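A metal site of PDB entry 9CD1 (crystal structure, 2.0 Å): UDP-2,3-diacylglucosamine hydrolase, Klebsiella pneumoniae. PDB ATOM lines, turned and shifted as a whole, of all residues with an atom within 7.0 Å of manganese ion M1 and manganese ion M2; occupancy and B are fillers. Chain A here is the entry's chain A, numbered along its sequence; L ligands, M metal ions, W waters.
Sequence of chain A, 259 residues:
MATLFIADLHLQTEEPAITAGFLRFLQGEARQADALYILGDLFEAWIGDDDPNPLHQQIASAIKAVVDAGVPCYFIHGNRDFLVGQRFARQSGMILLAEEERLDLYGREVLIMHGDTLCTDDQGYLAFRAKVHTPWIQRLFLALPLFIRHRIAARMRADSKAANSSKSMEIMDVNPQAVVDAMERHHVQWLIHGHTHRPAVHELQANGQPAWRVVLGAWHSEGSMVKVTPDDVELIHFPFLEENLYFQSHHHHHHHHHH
The guanidinium group of Arg 80 is in hydrogen-bond range of an oxygen (O4) of the ligand (2.8 Å).
ND2 of Asn 79 lies within hydrogen-bond range of O3 of the ligand (2.9 Å).
The side-chain carboxylate of Glu 44 lies within hydrogen-bond range of a ring nitrogen (ND1) of His 10.
The backbone carbonyl oxygen (O) of Asp 41 is in hydrogen-bond range of the backbone NH (N) of Leu 9 (3.0 Å).
The side-chain carboxylate of Asp 8 sits at hydrogen-bond distance from the backbone NH of His 195, 2.7 Å away.
The backbone NH (N) of Gly 194 lies within hydrogen-bond range of the backbone carbonyl oxygen (O) of His 114, 2.9 Å away.
The side-chain carboxylate of Asp 41 lies within hydrogen-bond range of the backbone NH of Arg 80 (3.1 Å).
The backbone NH (N) of Asp 8 is in hydrogen-bond range of the backbone carbonyl oxygen (O) of Gly 40, 3.0 Å away.
A ring nitrogen (ND1) of His 114 sits at hydrogen-bond distance from the backbone carbonyl oxygen of Leu 39.
Of the 21 residues printed, 4 come within 4 Å of manganese ion M2.
Manganese ion M1 is bound by OD1 of Asn 79 (2.0 Å), water W2 (2.1 Å), OD2 of Asp 41 (2.2 Å), NE2 of His 114 (2.2 Å) and ND1 of His 195 (2.4 Å).
Manganese ion M2 is bound by water W2, OD1 of Asp 8, NE2 of His 10, NE2 of His 197 and OD2 of Asp 41.
Water W1 lies within hydrogen-bond range of the side-chain amide nitrogen (ND2) of Asn 79 (3.0 Å) and an oxygen (O5) of the ligand (3.1 Å).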
ATOM      1  N   ALA A   7      10.633 -26.160 -35.809  1.00  0.00           N
ATOM      2  CA  ALA A   7       9.586 -25.458 -35.074  1.00  0.00           C
ATOM      3  C   ALA A   7      10.009 -24.002 -34.881  1.00  0.00           C
ATOM      4  O   ALA A   7      11.162 -23.639 -35.119  1.00  0.00           O
ATOM      5  CB  ALA A   7       9.308 -26.106 -33.711  1.00  0.00           C
ATOM      6  N   ASP A   8       9.038 -23.188 -34.459  1.00  0.00           N
ATOM      7  CA  ASP A   8       9.291 -21.817 -34.031  1.00  0.00           C
ATOM      8  C   ASP A   8       9.951 -20.988 -35.131  1.00  0.00           C
ATOM      9  O   ASP A   8      10.896 -20.230 -34.887  1.00  0.00           O
ATOM     10  CB  ASP A   8      10.118 -21.800 -32.746  1.00  0.00           C
ATOM     11  CG  ASP A   8       9.405 -22.481 -31.595  1.00  0.00           C
ATOM     12  OD1 ASP A   8       8.375 -21.947 -31.138  1.00  0.00           O
ATOM     13  OD2 ASP A   8       9.850 -23.568 -31.175  1.00  0.00           O
ATOM     14  N   LEU A   9       9.443 -21.126 -36.358  1.00  0.00           N
ATOM     15  CA  LEU A   9       9.895 -20.272 -37.451  1.00  0.00           C
ATOM     16  C   LEU A   9       9.284 -18.882 -37.348  1.00  0.00           C
ATOM     17  O   LEU A   9       9.914 -17.897 -37.737  1.00  0.00           O
ATOM     18  CB  LEU A   9       9.555 -20.920 -38.785  1.00  0.00           C
ATOM     19  CG  LEU A   9      10.454 -22.072 -39.248  1.00  0.00           C
ATOM     20  CD1 LEU A   9      10.032 -23.391 -38.617  1.00  0.00           C
ATOM     21  CD2 LEU A   9      10.416 -22.169 -40.764  1.00  0.00           C
ATOM     22  N   HIS A  10       8.052 -18.790 -36.841  1.00  0.00           N
ATOM     23  CA  HIS A  10       7.356 -17.516 -36.657  1.00  0.00           C
ATOM     24  C   HIS A  10       7.339 -16.704 -37.951  1.00  0.00           C
ATOM     25  O   HIS A  10       7.681 -15.518 -37.982  1.00  0.00           O
ATOM     26  CB  HIS A  10       7.993 -16.702 -35.514  1.00  0.00           C
ATOM     27  CG  HIS A  10       7.894 -17.372 -34.174  1.00  0.00           C
ATOM     28  ND1 HIS A  10       6.837 -17.160 -33.312  1.00  0.00           N
ATOM     29  CD2 HIS A  10       8.714 -18.245 -33.556  1.00  0.00           C
ATOM     30  CE1 HIS A  10       7.014 -17.878 -32.220  1.00  0.00           C
ATOM     31  NE2 HIS A  10       8.152 -18.547 -32.342  1.00  0.00           N
ATOM     32  N   LEU A  39       6.772 -28.800 -35.471  1.00  0.00           N
ATOM     33  CA  LEU A  39       6.238 -28.876 -34.115  1.00  0.00           C
ATOM     34  C   LEU A  39       5.753 -27.537 -33.587  1.00  0.00           C
ATOM     35  O   LEU A  39       6.043 -27.180 -32.440  1.00  0.00           O
ATOM     36  CB  LEU A  39       7.312 -29.460 -33.197  1.00  0.00           C
ATOM     37  CG  LEU A  39       7.885 -30.823 -33.581  1.00  0.00           C
ATOM     38  CD1 LEU A  39       8.792 -31.348 -32.481  1.00  0.00           C
ATOM     39  CD2 LEU A  39       6.769 -31.816 -33.887  1.00  0.00           C
ATOM     40  N   GLY A  40       4.996 -26.771 -34.370  1.00  0.00           N
ATOM     41  CA  GLY A  40       4.312 -25.622 -33.839  1.00  0.00           C
ATOM     42  C   GLY A  40       5.055 -24.320 -34.096  1.00  0.00           C
ATOM     43  O   GLY A  40       6.265 -24.286 -34.304  1.00  0.00           O
ATOM     44  N   ASP A  41       4.285 -23.224 -34.051  1.00  0.00           N
ATOM     45  CA  ASP A  41       4.803 -21.879 -34.285  1.00  0.00           C
ATOM     46  C   ASP A  41       5.469 -21.764 -35.657  1.00  0.00           C
ATOM     47  O   ASP A  41       6.516 -21.110 -35.805  1.00  0.00           O
ATOM     48  CB  ASP A  41       5.756 -21.446 -33.161  1.00  0.00           C
ATOM     49  CG  ASP A  41       5.031 -21.087 -31.880  1.00  0.00           C
ATOM     50  OD1 ASP A  41       3.786 -21.245 -31.830  1.00  0.00           O
ATOM     51  OD2 ASP A  41       5.699 -20.664 -30.924  1.00  0.00           O
ATOM     52  N   GLU A  44       3.882 -16.697 -37.173  1.00  0.00           N
ATOM     53  CA  GLU A  44       3.830 -15.796 -36.035  1.00  0.00           C
ATOM     54  C   GLU A  44       2.395 -15.578 -35.557  1.00  0.00           C
ATOM     55  O   GLU A  44       2.166 -15.306 -34.368  1.00  0.00           O
ATOM     56  CB  GLU A  44       4.491 -14.458 -36.388  1.00  0.00           C
ATOM     57  CG  GLU A  44       4.326 -13.346 -35.357  1.00  0.00           C
ATOM     58  CD  GLU A  44       5.013 -13.625 -34.030  1.00  0.00           C
ATOM     59  OE1 GLU A  44       5.805 -14.581 -33.931  1.00  0.00           O
ATOM     60  OE2 GLU A  44       4.747 -12.877 -33.060  1.00  0.00           O
ATOM     61  N   GLY A  78       1.279 -24.837 -32.469  1.00  0.00           N
ATOM     62  CA  GLY A  78       1.908 -24.046 -31.437  1.00  0.00           C
ATOM     63  C   GLY A  78       0.927 -23.078 -30.793  1.00  0.00           C
ATOM     64  O   GLY A  78      -0.260 -23.051 -31.106  1.00  0.00           O
ATOM     65  N   ASN A  79       1.452 -22.277 -29.870  1.00  0.00           N
ATOM     66  CA  ASN A  79       0.608 -21.279 -29.223  1.00  0.00           C
ATOM     67  C   ASN A  79       0.318 -20.090 -30.141  1.00  0.00           C
ATOM     68  O   ASN A  79      -0.664 -19.374 -29.902  1.00  0.00           O
ATOM     69  CB  ASN A  79       1.245 -20.784 -27.932  1.00  0.00           C
ATOM     70  CG  ASN A  79       2.645 -20.239 -28.133  1.00  0.00           C
ATOM     71  OD1 ASN A  79       3.563 -20.987 -28.480  1.00  0.00           O
ATOM     72  ND2 ASN A  79       2.809 -18.938 -27.926  1.00  0.00           N
ATOM     73  N   ARG A  80       1.137 -19.867 -31.170  1.00  0.00           N
ATOM     74  CA  ARG A  80       0.894 -18.764 -32.086  1.00  0.00           C
ATOM     75  C   ARG A  80      -0.100 -19.145 -33.184  1.00  0.00           C
ATOM     76  O   ARG A  80      -0.929 -18.325 -33.579  1.00  0.00           O
ATOM     77  CB  ARG A  80       2.210 -18.290 -32.713  1.00  0.00           C
ATOM     78  CG  ARG A  80       3.277 -17.888 -31.691  1.00  0.00           C
ATOM     79  CD  ARG A  80       2.788 -16.775 -30.772  1.00  0.00           C
ATOM     80  NE  ARG A  80       2.453 -15.561 -31.503  1.00  0.00           N
ATOM     81  CZ  ARG A  80       2.213 -14.385 -30.932  1.00  0.00           C
ATOM     82  NH1 ARG A  80       2.265 -14.231 -29.617  1.00  0.00           N
ATOM     83  NH2 ARG A  80       1.926 -13.337 -31.700  1.00  0.00           N
ATOM     84  N   HIS A 114       4.668 -29.393 -29.063  1.00  0.00           N
ATOM     85  CA  HIS A 114       5.210 -28.038 -29.188  1.00  0.00           C
ATOM     86  C   HIS A 114       6.049 -27.671 -27.979  1.00  0.00           C
ATOM     87  O   HIS A 114       7.090 -27.019 -28.112  1.00  0.00           O
ATOM     88  CB  HIS A 114       4.080 -27.026 -29.381  1.00  0.00           C
ATOM     89  CG  HIS A 114       4.569 -25.622 -29.546  1.00  0.00           C
ATOM     90  ND1 HIS A 114       5.443 -25.252 -30.554  1.00  0.00           N
ATOM     91  CD2 HIS A 114       4.337 -24.500 -28.827  1.00  0.00           C
ATOM     92  CE1 HIS A 114       5.717 -23.962 -30.442  1.00  0.00           C
ATOM     93  NE2 HIS A 114       5.057 -23.481 -29.402  1.00  0.00           N
ATOM     94  N   GLY A 115       5.622 -28.076 -26.780  1.00  0.00           N
ATOM     95  CA  GLY A 115       6.365 -27.855 -25.562  1.00  0.00           C
ATOM     96  C   GLY A 115       5.744 -26.856 -24.615  1.00  0.00           C
ATOM     97  O   GLY A 115       6.176 -26.779 -23.456  1.00  0.00           O
ATOM     98  N   ASP A 116       4.742 -26.081 -25.053  1.00  0.00           N
ATOM     99  CA  ASP A 116       4.155 -25.087 -24.158  1.00  0.00           C
ATOM    100  C   ASP A 116       3.378 -25.737 -23.017  1.00  0.00           C
ATOM    101  O   ASP A 116       3.272 -25.142 -21.940  1.00  0.00           O
ATOM    102  CB  ASP A 116       3.240 -24.129 -24.942  1.00  0.00           C
ATOM    103  CG  ASP A 116       2.128 -24.854 -25.671  1.00  0.00           C
ATOM    104  OD1 ASP A 116       2.426 -25.787 -26.445  1.00  0.00           O
ATOM    105  OD2 ASP A 116       0.953 -24.487 -25.460  1.00  0.00           O
ATOM    106  N   TYR A 125      -0.228 -17.938 -18.792  1.00  0.00           N
ATOM    107  CA  TYR A 125      -0.340 -18.452 -20.147  1.00  0.00           C
ATOM    108  C   TYR A 125      -1.290 -19.643 -20.208  1.00  0.00           C
ATOM    109  O   TYR A 125      -2.054 -19.793 -21.173  1.00  0.00           O
ATOM    110  CB  TYR A 125       1.029 -18.866 -20.695  1.00  0.00           C
ATOM    111  CG  TYR A 125       0.889 -19.747 -21.915  1.00  0.00           C
ATOM    112  CD1 TYR A 125       0.454 -19.220 -23.123  1.00  0.00           C
ATOM    113  CD2 TYR A 125       1.138 -21.115 -21.835  1.00  0.00           C
ATOM    114  CE1 TYR A 125       0.303 -20.027 -24.234  1.00  0.00           C
ATOM    115  CE2 TYR A 125       0.992 -21.923 -22.938  1.00  0.00           C
ATOM    116  CZ  TYR A 125       0.569 -21.376 -24.139  1.00  0.00           C
ATOM    117  OH  TYR A 125       0.418 -22.178 -25.237  1.00  0.00           O
ATOM    118  N   ILE A 171       9.791 -15.861 -22.911  1.00  0.00           N
ATOM    119  CA  ILE A 171       9.139 -17.156 -22.771  1.00  0.00           C
ATOM    120  C   ILE A 171       9.738 -17.919 -21.596  1.00  0.00           C
ATOM    121  O   ILE A 171      10.948 -18.118 -21.530  1.00  0.00           O
ATOM    122  CB  ILE A 171       9.240 -17.980 -24.058  1.00  0.00           C
ATOM    123  CG1 ILE A 171       8.761 -17.160 -25.261  1.00  0.00           C
ATOM    124  CG2 ILE A 171       8.438 -19.264 -23.942  1.00  0.00           C
ATOM    125  CD1 ILE A 171       9.165 -17.743 -26.593  1.00  0.00           C
ATOM    126  N   GLY A 194       9.717 -27.724 -29.057  1.00  0.00           N
ATOM    127  CA  GLY A 194      10.223 -26.380 -29.246  1.00  0.00           C
ATOM    128  C   GLY A 194       9.667 -25.423 -28.216  1.00  0.00           C
ATOM    129  O   GLY A 194       9.769 -25.672 -27.017  1.00  0.00           O
ATOM    130  N   HIS A 195       9.088 -24.313 -28.696  1.00  0.00           N
ATOM    131  CA  HIS A 195       8.414 -23.298 -27.883  1.00  0.00           C
ATOM    132  C   HIS A 195       9.365 -22.469 -27.018  1.00  0.00           C
ATOM    133  O   HIS A 195       9.246 -21.242 -26.979  1.00  0.00           O
ATOM    134  CB  HIS A 195       7.345 -23.931 -26.989  1.00  0.00           C
ATOM    135  CG  HIS A 195       6.655 -22.943 -26.105  1.00  0.00           C
ATOM    136  ND1 HIS A 195       5.789 -21.986 -26.588  1.00  0.00           N
ATOM    137  CD2 HIS A 195       6.718 -22.736 -24.765  1.00  0.00           C
ATOM    138  CE1 HIS A 195       5.339 -21.246 -25.585  1.00  0.00           C
ATOM    139  NE2 HIS A 195       5.893 -21.676 -24.473  1.00  0.00           N
ATOM    140  N   THR A 196      10.281 -23.115 -26.296  1.00  0.00           N
ATOM    141  CA  THR A 196      11.119 -22.379 -25.350  1.00  0.00           C
ATOM    142  C   THR A 196      12.246 -21.604 -26.026  1.00  0.00           C
ATOM    143  O   THR A 196      12.848 -20.741 -25.375  1.00  0.00           O
ATOM    144  CB  THR A 196      11.707 -23.322 -24.298  1.00  0.00           C
ATOM    145  OG1 THR A 196      12.527 -24.301 -24.938  1.00  0.00           O
ATOM    146  CG2 THR A 196      10.598 -24.007 -23.521  1.00  0.00           C
ATOM    147  N   HIS A 197      12.542 -21.891 -27.293  1.00  0.00           N
ATOM    148  CA  HIS A 197      13.571 -21.167 -28.055  1.00  0.00           C
ATOM    149  C   HIS A 197      14.948 -21.327 -27.416  1.00  0.00           C
ATOM    150  O   HIS A 197      15.796 -20.432 -27.517  1.00  0.00           O
ATOM    151  CB  HIS A 197      13.215 -19.687 -28.214  1.00  0.00           C
ATOM    152  CG  HIS A 197      11.934 -19.438 -28.946  1.00  0.00           C
ATOM    153  ND1 HIS A 197      11.522 -18.178 -29.324  1.00  0.00           N
ATOM    154  CD2 HIS A 197      10.976 -20.289 -29.396  1.00  0.00           C
ATOM    155  CE1 HIS A 197      10.367 -18.255 -29.953  1.00  0.00           C
ATOM    156  NE2 HIS A 197      10.013 -19.532 -30.016  1.00  0.00           N
ATOM    157  N   ALA A 218      14.534 -21.384 -32.343  1.00  0.00           N
ATOM    158  CA  ALA A 218      13.718 -20.503 -33.175  1.00  0.00           C
ATOM    159  C   ALA A 218      14.548 -19.977 -34.338  1.00  0.00           C
ATOM    160  O   ALA A 218      15.778 -19.877 -34.261  1.00  0.00           O
ATOM    161  CB  ALA A 218      13.163 -19.338 -32.350  1.00  0.00           C
HETATM  162  C1  LIG L   1      -6.313 -15.979 -32.626  1.00  0.00           C
HETATM  163  C2  LIG L   1      -1.587 -15.959 -30.701  1.00  0.00           C
HETATM  164  C3  LIG L   1      -1.005 -15.049 -28.537  1.00  0.00           C
HETATM  165  C4  LIG L   1       0.249 -16.251 -26.527  1.00  0.00           C
HETATM  166  C5  LIG L   1       1.810 -16.108 -24.434  1.00  0.00           C
HETATM  167  C6  LIG L   1       3.695 -17.717 -25.096  1.00  0.00           C
HETATM  168  C7  LIG L   1      -9.524 -17.161 -30.185  1.00  0.00           C
HETATM  169  C8  LIG L   1      -8.091 -15.499 -30.864  1.00  0.00           C
HETATM  170  C9  LIG L   1      -6.501 -13.723 -31.866  1.00  0.00           C
HETATM  171  C10 LIG L   1      -4.977 -13.618 -31.792  1.00  0.00           C
HETATM  172  C11 LIG L   1      -4.788 -15.902 -32.520  1.00  0.00           C
HETATM  173  C12 LIG L   1      -1.937 -14.670 -31.120  1.00  0.00           C
HETATM  174  C13 LIG L   1      -1.115 -16.152 -29.389  1.00  0.00           C
HETATM  175  C14 LIG L   1      -1.384 -13.781 -28.964  1.00  0.00           C
HETATM  176  C15 LIG L   1      -1.838 -13.583 -30.263  1.00  0.00           C
HETATM  177  C16 LIG L   1       0.527 -16.045 -25.008  1.00  0.00           C
HETATM  178  C17 LIG L   1       4.876 -14.181 -25.469  1.00  0.00           C
HETATM  179  C18 LIG L   1       1.948 -15.892 -23.060  1.00  0.00           C
HETATM  180  C19 LIG L   1       0.833 -15.597 -22.266  1.00  0.00           C
HETATM  181  C20 LIG L   1      -0.433 -15.519 -22.838  1.00  0.00           C
HETATM  182  C21 LIG L   1      -0.571 -15.735 -24.211  1.00  0.00           C
HETATM  183  C22 LIG L   1      -8.823 -14.541 -30.143  1.00  0.00           C
HETATM  184  C23 LIG L   1      -9.954 -14.950 -29.429  1.00  0.00           C
HETATM  185  C24 LIG L   1     -10.318 -16.293 -29.445  1.00  0.00           C
HETATM  186  C25 LIG L   1     -10.767 -13.914 -28.622  1.00  0.00           C
HETATM  187  F1  LIG L   1     -12.036 -14.378 -28.467  1.00  0.00           F
HETATM  188  F2  LIG L   1     -10.801 -12.720 -29.302  1.00  0.00           F
HETATM  189  F3  LIG L   1     -10.186 -13.716 -27.402  1.00  0.00           F
HETATM  190  N1  LIG L   1      -8.456 -16.745 -30.864  1.00  0.00           N
HETATM  191  N2  LIG L   1      -6.897 -15.108 -31.640  1.00  0.00           N
HETATM  192  N3  LIG L   1      -4.287 -14.547 -32.690  1.00  0.00           N
HETATM  193  N4  LIG L   1      -0.545 -15.168 -27.118  1.00  0.00           N
HETATM  194  N5  LIG L   1       3.012 -16.408 -25.242  1.00  0.00           N
HETATM  195  O1  LIG L   1      -2.037 -15.321 -33.796  1.00  0.00           O
HETATM  196  O2  LIG L   1      -2.211 -13.043 -33.330  1.00  0.00           O
HETATM  197  O3  LIG L   1       0.630 -17.187 -27.150  1.00  0.00           O
HETATM  198  O4  LIG L   1       2.554 -14.365 -26.872  1.00  0.00           O
HETATM  199  O5  LIG L   1       4.188 -15.810 -27.548  1.00  0.00           O
HETATM  200  S1  LIG L   1      -2.576 -14.370 -32.817  1.00  0.00           S
HETATM  201  S2  LIG L   1       3.633 -15.209 -26.327  1.00  0.00           S
HETATM  202 CL1  LIG L   1      -9.930 -18.896 -30.260  1.00  0.00          CL
HETATM  203 MN    MN M   1       5.463 -21.339 -28.859  1.00  0.00          MN
HETATM  204 MN    MN M   2       7.911 -20.048 -30.734  1.00  0.00          MN
HETATM  205  O   HOH W   1       5.675 -18.306 -28.665  1.00  0.00           O
HETATM  206  O   HOH W   2       7.209 -20.144 -28.894  1.00  0.00           O
